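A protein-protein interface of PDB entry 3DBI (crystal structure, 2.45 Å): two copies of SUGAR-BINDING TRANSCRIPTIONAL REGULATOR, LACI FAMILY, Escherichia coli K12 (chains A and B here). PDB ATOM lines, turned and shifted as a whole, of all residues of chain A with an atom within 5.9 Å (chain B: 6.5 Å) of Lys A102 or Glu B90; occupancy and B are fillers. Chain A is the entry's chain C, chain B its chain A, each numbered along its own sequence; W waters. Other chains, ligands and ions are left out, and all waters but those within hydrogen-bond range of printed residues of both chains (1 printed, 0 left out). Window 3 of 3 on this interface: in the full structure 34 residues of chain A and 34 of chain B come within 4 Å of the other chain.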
ATOM      1  N   VAL A  68      -2.165 -19.207   4.762  1.00  0.00           N
ATOM      2  CA  VAL A  68      -0.871 -18.648   5.131  1.00  0.00           C
ATOM      3  C   VAL A  68      -0.901 -17.165   4.808  1.00  0.00           C
ATOM      4  O   VAL A  68      -1.105 -16.787   3.653  1.00  0.00           O
ATOM      5  CB  VAL A  68       0.284 -19.323   4.355  1.00  0.00           C
ATOM      6  CG1 VAL A  68       1.639 -18.827   4.854  1.00  0.00           C
ATOM      7  CG2 VAL A  68       0.197 -20.834   4.486  1.00  0.00           C
ATOM      8  N   THR A  69      -0.708 -16.332   5.827  1.00  0.00           N
ATOM      9  CA  THR A  69      -0.709 -14.877   5.644  1.00  0.00           C
ATOM     10  C   THR A  69       0.657 -14.253   5.917  1.00  0.00           C
ATOM     11  O   THR A  69       1.553 -14.897   6.478  1.00  0.00           O
ATOM     12  CB  THR A  69      -1.775 -14.178   6.534  1.00  0.00           C
ATOM     13  OG1 THR A  69      -1.586 -14.556   7.903  1.00  0.00           O
ATOM     14  CG2 THR A  69      -3.197 -14.561   6.096  1.00  0.00           C
ATOM     15  N   ASN A  70       0.795 -12.988   5.529  1.00  0.00           N
ATOM     16  CA  ASN A  70       2.012 -12.204   5.748  1.00  0.00           C
ATOM     17  C   ASN A  70       2.191 -11.807   7.227  1.00  0.00           C
ATOM     18  O   ASN A  70       2.359 -10.634   7.564  1.00  0.00           O
ATOM     19  CB  ASN A  70       1.978 -10.961   4.847  1.00  0.00           C
ATOM     20  CG  ASN A  70       3.363 -10.467   4.463  1.00  0.00           C
ATOM     21  OD1 ASN A  70       4.365 -11.163   4.645  1.00  0.00           O
ATOM     22  ND2 ASN A  70       3.420  -9.259   3.911  1.00  0.00           N
ATOM     23  N   ASP A 100      -1.954 -20.000   0.041  1.00  0.00           N
ATOM     24  CA  ASP A 100      -1.168 -18.787   0.123  1.00  0.00           C
ATOM     25  C   ASP A 100      -2.072 -17.557   0.002  1.00  0.00           C
ATOM     26  O   ASP A 100      -2.717 -17.348  -1.026  1.00  0.00           O
ATOM     27  CB  ASP A 100      -0.095 -18.791  -0.968  1.00  0.00           C
ATOM     28  CG  ASP A 100       0.882 -17.634  -0.843  1.00  0.00           C
ATOM     29  OD1 ASP A 100       0.967 -17.021   0.246  1.00  0.00           O
ATOM     30  OD2 ASP A 100       1.572 -17.344  -1.842  1.00  0.00           O
ATOM     31  N   GLY A 101      -2.107 -16.748   1.058  1.00  0.00           N
ATOM     32  CA  GLY A 101      -2.924 -15.533   1.081  1.00  0.00           C
ATOM     33  C   GLY A 101      -2.237 -14.333   0.446  1.00  0.00           C
ATOM     34  O   GLY A 101      -2.869 -13.295   0.216  1.00  0.00           O
ATOM     35  N   LYS A 102      -0.941 -14.489   0.177  1.00  0.00           N
ATOM     36  CA  LYS A 102      -0.110 -13.500  -0.511  1.00  0.00           C
ATOM     37  C   LYS A 102      -0.125 -12.125   0.146  1.00  0.00           C
ATOM     38  O   LYS A 102       0.081 -12.011   1.354  1.00  0.00           O
ATOM     39  CB  LYS A 102      -0.468 -13.402  -1.998  1.00  0.00           C
ATOM     40  CG  LYS A 102      -0.414 -14.707  -2.754  1.00  0.00           C
ATOM     41  CD  LYS A 102      -0.717 -14.490  -4.219  1.00  0.00           C
ATOM     42  CE  LYS A 102      -0.886 -15.798  -4.962  1.00  0.00           C
ATOM     43  NZ  LYS A 102       0.364 -16.624  -4.975  1.00  0.00           N
ATOM     44  N   HIS A 103      -0.393 -11.088  -0.646  1.00  0.00           N
ATOM     45  CA  HIS A 103      -0.089  -9.724  -0.227  1.00  0.00           C
ATOM     46  C   HIS A 103      -1.190  -8.664  -0.412  1.00  0.00           C
ATOM     47  O   HIS A 103      -0.884  -7.473  -0.482  1.00  0.00           O
ATOM     48  CB  HIS A 103       1.206  -9.262  -0.911  1.00  0.00           C
ATOM     49  CG  HIS A 103       2.422 -10.019  -0.476  1.00  0.00           C
ATOM     50  ND1 HIS A 103       2.997 -11.008  -1.244  1.00  0.00           N
ATOM     51  CD2 HIS A 103       3.164  -9.942   0.656  1.00  0.00           C
ATOM     52  CE1 HIS A 103       4.046 -11.501  -0.611  1.00  0.00           C
ATOM     53  NE2 HIS A 103       4.169 -10.872   0.545  1.00  0.00           N
ATOM     54  N   SER A 104      -2.453  -9.082  -0.463  1.00  0.00           N
ATOM     55  CA  SER A 104      -3.582  -8.141  -0.531  1.00  0.00           C
ATOM     56  C   SER A 104      -4.861  -8.754   0.024  1.00  0.00           C
ATOM     57  O   SER A 104      -4.914  -9.963   0.278  1.00  0.00           O
ATOM     58  CB  SER A 104      -3.821  -7.679  -1.971  1.00  0.00           C
ATOM     59  OG  SER A 104      -4.247  -8.759  -2.774  1.00  0.00           O
ATOM     60  N   GLU A 107      -6.297 -11.188  -2.609  1.00  0.00           N
ATOM     61  CA  GLU A 107      -5.550 -12.444  -2.592  1.00  0.00           C
ATOM     62  C   GLU A 107      -5.860 -13.315  -1.365  1.00  0.00           C
ATOM     63  O   GLU A 107      -5.883 -14.542  -1.483  1.00  0.00           O
ATOM     64  CB  GLU A 107      -4.048 -12.187  -2.711  1.00  0.00           C
ATOM     65  CG  GLU A 107      -3.589 -11.780  -4.113  1.00  0.00           C
ATOM     66  CD  GLU A 107      -2.220 -11.103  -4.119  1.00  0.00           C
ATOM     67  OE1 GLU A 107      -1.922 -10.304  -3.200  1.00  0.00           O
ATOM     68  OE2 GLU A 107      -1.439 -11.370  -5.053  1.00  0.00           O
ATOM     69  N   GLU A 108      -6.107 -12.680  -0.213  1.00  0.00           N
ATOM     70  CA  GLU A 108      -6.531 -13.396   0.996  1.00  0.00           C
ATOM     71  C   GLU A 108      -7.917 -14.014   0.835  1.00  0.00           C
ATOM     72  O   GLU A 108      -8.149 -15.148   1.262  1.00  0.00           O
ATOM     73  CB  GLU A 108      -6.471 -12.498   2.234  1.00  0.00           C
ATOM     74  CG  GLU A 108      -5.052 -12.341   2.791  1.00  0.00           C
ATOM     75  CD  GLU A 108      -4.979 -11.588   4.113  1.00  0.00           C
ATOM     76  OE1 GLU A 108      -6.019 -11.096   4.601  1.00  0.00           O
ATOM     77  OE2 GLU A 108      -3.864 -11.490   4.669  1.00  0.00           O
ATOM     78  N   PHE A 129      -4.657  -8.284   5.614  1.00  0.00           N
ATOM     79  CA  PHE A 129      -5.288  -7.279   4.766  1.00  0.00           C
ATOM     80  C   PHE A 129      -6.807  -7.326   4.798  1.00  0.00           C
ATOM     81  O   PHE A 129      -7.450  -6.279   4.801  1.00  0.00           O
ATOM     82  CB  PHE A 129      -4.824  -7.417   3.316  1.00  0.00           C
ATOM     83  CG  PHE A 129      -3.363  -7.152   3.107  1.00  0.00           C
ATOM     84  CD1 PHE A 129      -2.894  -5.850   2.947  1.00  0.00           C
ATOM     85  CD2 PHE A 129      -2.453  -8.209   3.043  1.00  0.00           C
ATOM     86  CE1 PHE A 129      -1.537  -5.597   2.745  1.00  0.00           C
ATOM     87  CE2 PHE A 129      -1.093  -7.969   2.845  1.00  0.00           C
ATOM     88  CZ  PHE A 129      -0.634  -6.658   2.691  1.00  0.00           C
ATOM     89  N   PHE B  83       6.708 -20.672   3.982  1.00  0.00           N
ATOM     90  CA  PHE B  83       6.351 -19.521   3.146  1.00  0.00           C
ATOM     91  C   PHE B  83       6.585 -19.824   1.670  1.00  0.00           C
ATOM     92  O   PHE B  83       5.657 -19.757   0.869  1.00  0.00           O
ATOM     93  CB  PHE B  83       7.141 -18.275   3.588  1.00  0.00           C
ATOM     94  CG  PHE B  83       6.832 -17.022   2.796  1.00  0.00           C
ATOM     95  CD1 PHE B  83       5.681 -16.273   3.061  1.00  0.00           C
ATOM     96  CD2 PHE B  83       7.715 -16.565   1.812  1.00  0.00           C
ATOM     97  CE1 PHE B  83       5.400 -15.107   2.343  1.00  0.00           C
ATOM     98  CE2 PHE B  83       7.441 -15.401   1.086  1.00  0.00           C
ATOM     99  CZ  PHE B  83       6.282 -14.672   1.354  1.00  0.00           C
ATOM    100  N   ALA B  85       7.320 -22.702   0.170  1.00  0.00           N
ATOM    101  CA  ALA B  85       6.593 -23.889  -0.292  1.00  0.00           C
ATOM    102  C   ALA B  85       5.134 -23.571  -0.598  1.00  0.00           C
ATOM    103  O   ALA B  85       4.573 -24.107  -1.553  1.00  0.00           O
ATOM    104  CB  ALA B  85       6.680 -25.025   0.710  1.00  0.00           C
ATOM    105  N   ALA B  86       4.528 -22.705   0.212  1.00  0.00           N
ATOM    106  CA  ALA B  86       3.180 -22.223  -0.053  1.00  0.00           C
ATOM    107  C   ALA B  86       3.097 -21.419  -1.344  1.00  0.00           C
ATOM    108  O   ALA B  86       2.146 -21.587  -2.104  1.00  0.00           O
ATOM    109  CB  ALA B  86       2.662 -21.406   1.109  1.00  0.00           C
ATOM    110  N   ARG B  87       4.092 -20.564  -1.574  1.00  0.00           N
ATOM    111  CA  ARG B  87       4.167 -19.726  -2.766  1.00  0.00           C
ATOM    112  C   ARG B  87       4.348 -20.557  -4.036  1.00  0.00           C
ATOM    113  O   ARG B  87       3.642 -20.336  -5.024  1.00  0.00           O
ATOM    114  CB  ARG B  87       5.295 -18.703  -2.633  1.00  0.00           C
ATOM    115  CG  ARG B  87       5.227 -17.540  -3.621  1.00  0.00           C
ATOM    116  CD  ARG B  87       5.760 -16.259  -2.986  1.00  0.00           C
ATOM    117  NE  ARG B  87       4.974 -15.903  -1.805  1.00  0.00           N
ATOM    118  CZ  ARG B  87       4.068 -14.930  -1.755  1.00  0.00           C
ATOM    119  NH1 ARG B  87       3.829 -14.170  -2.818  1.00  0.00           N
ATOM    120  NH2 ARG B  87       3.404 -14.711  -0.629  1.00  0.00           N
ATOM    121  N   MET B  88       5.276 -21.514  -3.989  1.00  0.00           N
ATOM    122  CA  MET B  88       5.575 -22.371  -5.128  1.00  0.00           C
ATOM    123  C   MET B  88       4.368 -23.208  -5.515  1.00  0.00           C
ATOM    124  O   MET B  88       4.013 -23.277  -6.695  1.00  0.00           O
ATOM    125  CB  MET B  88       6.775 -23.271  -4.832  1.00  0.00           C
ATOM    126  CG  MET B  88       7.206 -24.113  -6.012  1.00  0.00           C
ATOM    127  SD  MET B  88       6.452 -25.897  -5.969  1.00  0.00           S
ATOM    128  CE  MET B  88       7.964 -26.701  -5.023  1.00  0.00           C
ATOM    129  N   ALA B  89       3.740 -23.823  -4.515  1.00  0.00           N
ATOM    130  CA  ALA B  89       2.536 -24.637  -4.713  1.00  0.00           C
ATOM    131  C   ALA B  89       1.406 -23.884  -5.423  1.00  0.00           C
ATOM    132  O   ALA B  89       0.734 -24.435  -6.299  1.00  0.00           O
ATOM    133  CB  ALA B  89       2.047 -25.185  -3.387  1.00  0.00           C
ATOM    134  N   GLU B  90       1.213 -22.623  -5.047  1.00  0.00           N
ATOM    135  CA  GLU B  90       0.195 -21.790  -5.659  1.00  0.00           C
ATOM    136  C   GLU B  90       0.580 -21.421  -7.092  1.00  0.00           C
ATOM    137  O   GLU B  90      -0.254 -21.516  -7.992  1.00  0.00           O
ATOM    138  CB  GLU B  90      -0.062 -20.543  -4.809  1.00  0.00           C
ATOM    139  CG  GLU B  90      -1.460 -19.952  -4.968  1.00  0.00           C
ATOM    140  CD  GLU B  90      -1.624 -19.101  -6.228  1.00  0.00           C
ATOM    141  OE1 GLU B  90      -0.611 -18.546  -6.722  1.00  0.00           O
ATOM    142  OE2 GLU B  90      -2.770 -18.989  -6.725  1.00  0.00           O
ATOM    143  N   GLU B  91       1.838 -21.017  -7.288  1.00  0.00           N
ATOM    144  CA  GLU B  91       2.367 -20.649  -8.607  1.00  0.00           C
ATOM    145  C   GLU B  91       2.330 -21.799  -9.614  1.00  0.00           C
ATOM    146  O   GLU B  91       2.102 -21.576 -10.801  1.00  0.00           O
ATOM    147  CB  GLU B  91       3.801 -20.122  -8.487  1.00  0.00           C
ATOM    148  CG  GLU B  91       3.914 -18.705  -7.935  1.00  0.00           C
ATOM    149  CD  GLU B  91       5.354 -18.269  -7.664  1.00  0.00           C
ATOM    150  OE1 GLU B  91       6.301 -18.958  -8.107  1.00  0.00           O
ATOM    151  OE2 GLU B  91       5.534 -17.223  -7.006  1.00  0.00           O
ATOM    152  N   LYS B  92       2.550 -23.019  -9.131  1.00  0.00           N
ATOM    153  CA  LYS B  92       2.586 -24.206  -9.983  1.00  0.00           C
ATOM    154  C   LYS B  92       1.245 -24.941  -9.987  1.00  0.00           C
ATOM    155  O   LYS B  92       1.098 -25.976 -10.636  1.00  0.00           O
ATOM    156  CB  LYS B  92       3.734 -25.140  -9.560  1.00  0.00           C
ATOM    157  CG  LYS B  92       5.144 -24.611  -9.868  1.00  0.00           C
ATOM    158  CD  LYS B  92       5.413 -24.559 -11.377  1.00  0.00           C
ATOM    159  CE  LYS B  92       6.862 -24.215 -11.700  1.00  0.00           C
ATOM    160  NZ  LYS B  92       7.206 -22.824 -11.321  1.00  0.00           N
ATOM    161  N   GLY B  93       0.275 -24.389  -9.261  1.00  0.00           N
ATOM    162  CA  GLY B  93      -1.090 -24.920  -9.225  1.00  0.00           C
ATOM    163  C   GLY B  93      -1.277 -26.250  -8.508  1.00  0.00           C
ATOM    164  O   GLY B  93      -2.162 -27.022  -8.863  1.00  0.00           O
ATOM    165  N   ARG B  94      -0.455 -26.521  -7.498  1.00  0.00           N
ATOM    166  CA  ARG B  94      -0.586 -27.760  -6.723  1.00  0.00           C
ATOM    167  C   ARG B  94      -1.029 -27.544  -5.267  1.00  0.00           C
ATOM    168  O   ARG B  94      -0.830 -26.471  -4.694  1.00  0.00           O
ATOM    169  CB  ARG B  94       0.677 -28.636  -6.828  1.00  0.00           C
ATOM    170  CG  ARG B  94       2.001 -27.953  -6.559  1.00  0.00           C
ATOM    171  CD  ARG B  94       3.054 -28.343  -7.598  1.00  0.00           C
ATOM    172  NE  ARG B  94       3.145 -29.788  -7.808  1.00  0.00           N
ATOM    173  CZ  ARG B  94       3.882 -30.369  -8.752  1.00  0.00           C
ATOM    174  NH1 ARG B  94       3.892 -31.689  -8.858  1.00  0.00           N
ATOM    175  NH2 ARG B  94       4.609 -29.638  -9.591  1.00  0.00           N
HETATM  176  O   HOH W   1      -0.587 -22.108  -1.748  1.00  0.00           O
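The side-chain carboxylate of Asp A100 lies within salt-bridge range of the guanidinium group of Arg B87 (3.4 Å).
The side-chain amino group (NZ) of Lys A102 is in salt-bridge range of the side-chain carboxylate (OE1) of Glu B90, at 2.8 Å.
No position is printed for both chains.
Of the 5 pairs that touch across the chains among the printed residues, none has its exchanged pair printed and touching as well.
Of the printed residues of chain B, Asp A100 touches Ala B86 (3.8 Å) and Arg B87 (3.4 Å).
Printed residues of chain B within 4 Å of Lys A102: Arg B87 and Glu B90.
Of the printed residues of chain B, His A103 touches Arg B87 (3.3 Å).
Glu A107 touches none of the printed residues of chain B.
Printed residues of chain A within 4 Å of Ala B86: Asp A100 (3.8 Å).
Of the printed residues of chain A, Arg B87 touches Asp A100, Lys A102 and His A103.
Glu B90 touches just one residue of chain A: Lys A102.
The nearest residue of chain A that does not touch Glu B90 is Asp A100 (4.2 Å).
Of the 11 printed residues of chain A, 3 touch a printed residue of chain B.
Hydrophobic or aromatic side chains of chain A that line the printed part of chain B: His A103.
Printed residues of chain B that touch a printed residue of chain A: Ala B86, Arg B87 and Glu B90.
Among the printed residues, 5 pairs touch across the chains.
The side-chain amino group (NZ) of Lys A102 is in salt-bridge range of the side-chain carboxylate (OD2) of Asp A100, 3.4 Å away.
N of His A103 is in hydrogen-bond range of OE1 of Glu A107.
Asp A100 touches Ala B86.
Lys A102 touches Arg B87.
NH2 of Arg B87 touches CE1 of His A103 (3.3 Å).
Water W1 bridges O of Ala B86 (2.8 Å) and N of Asp A100 (3.1 Å).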
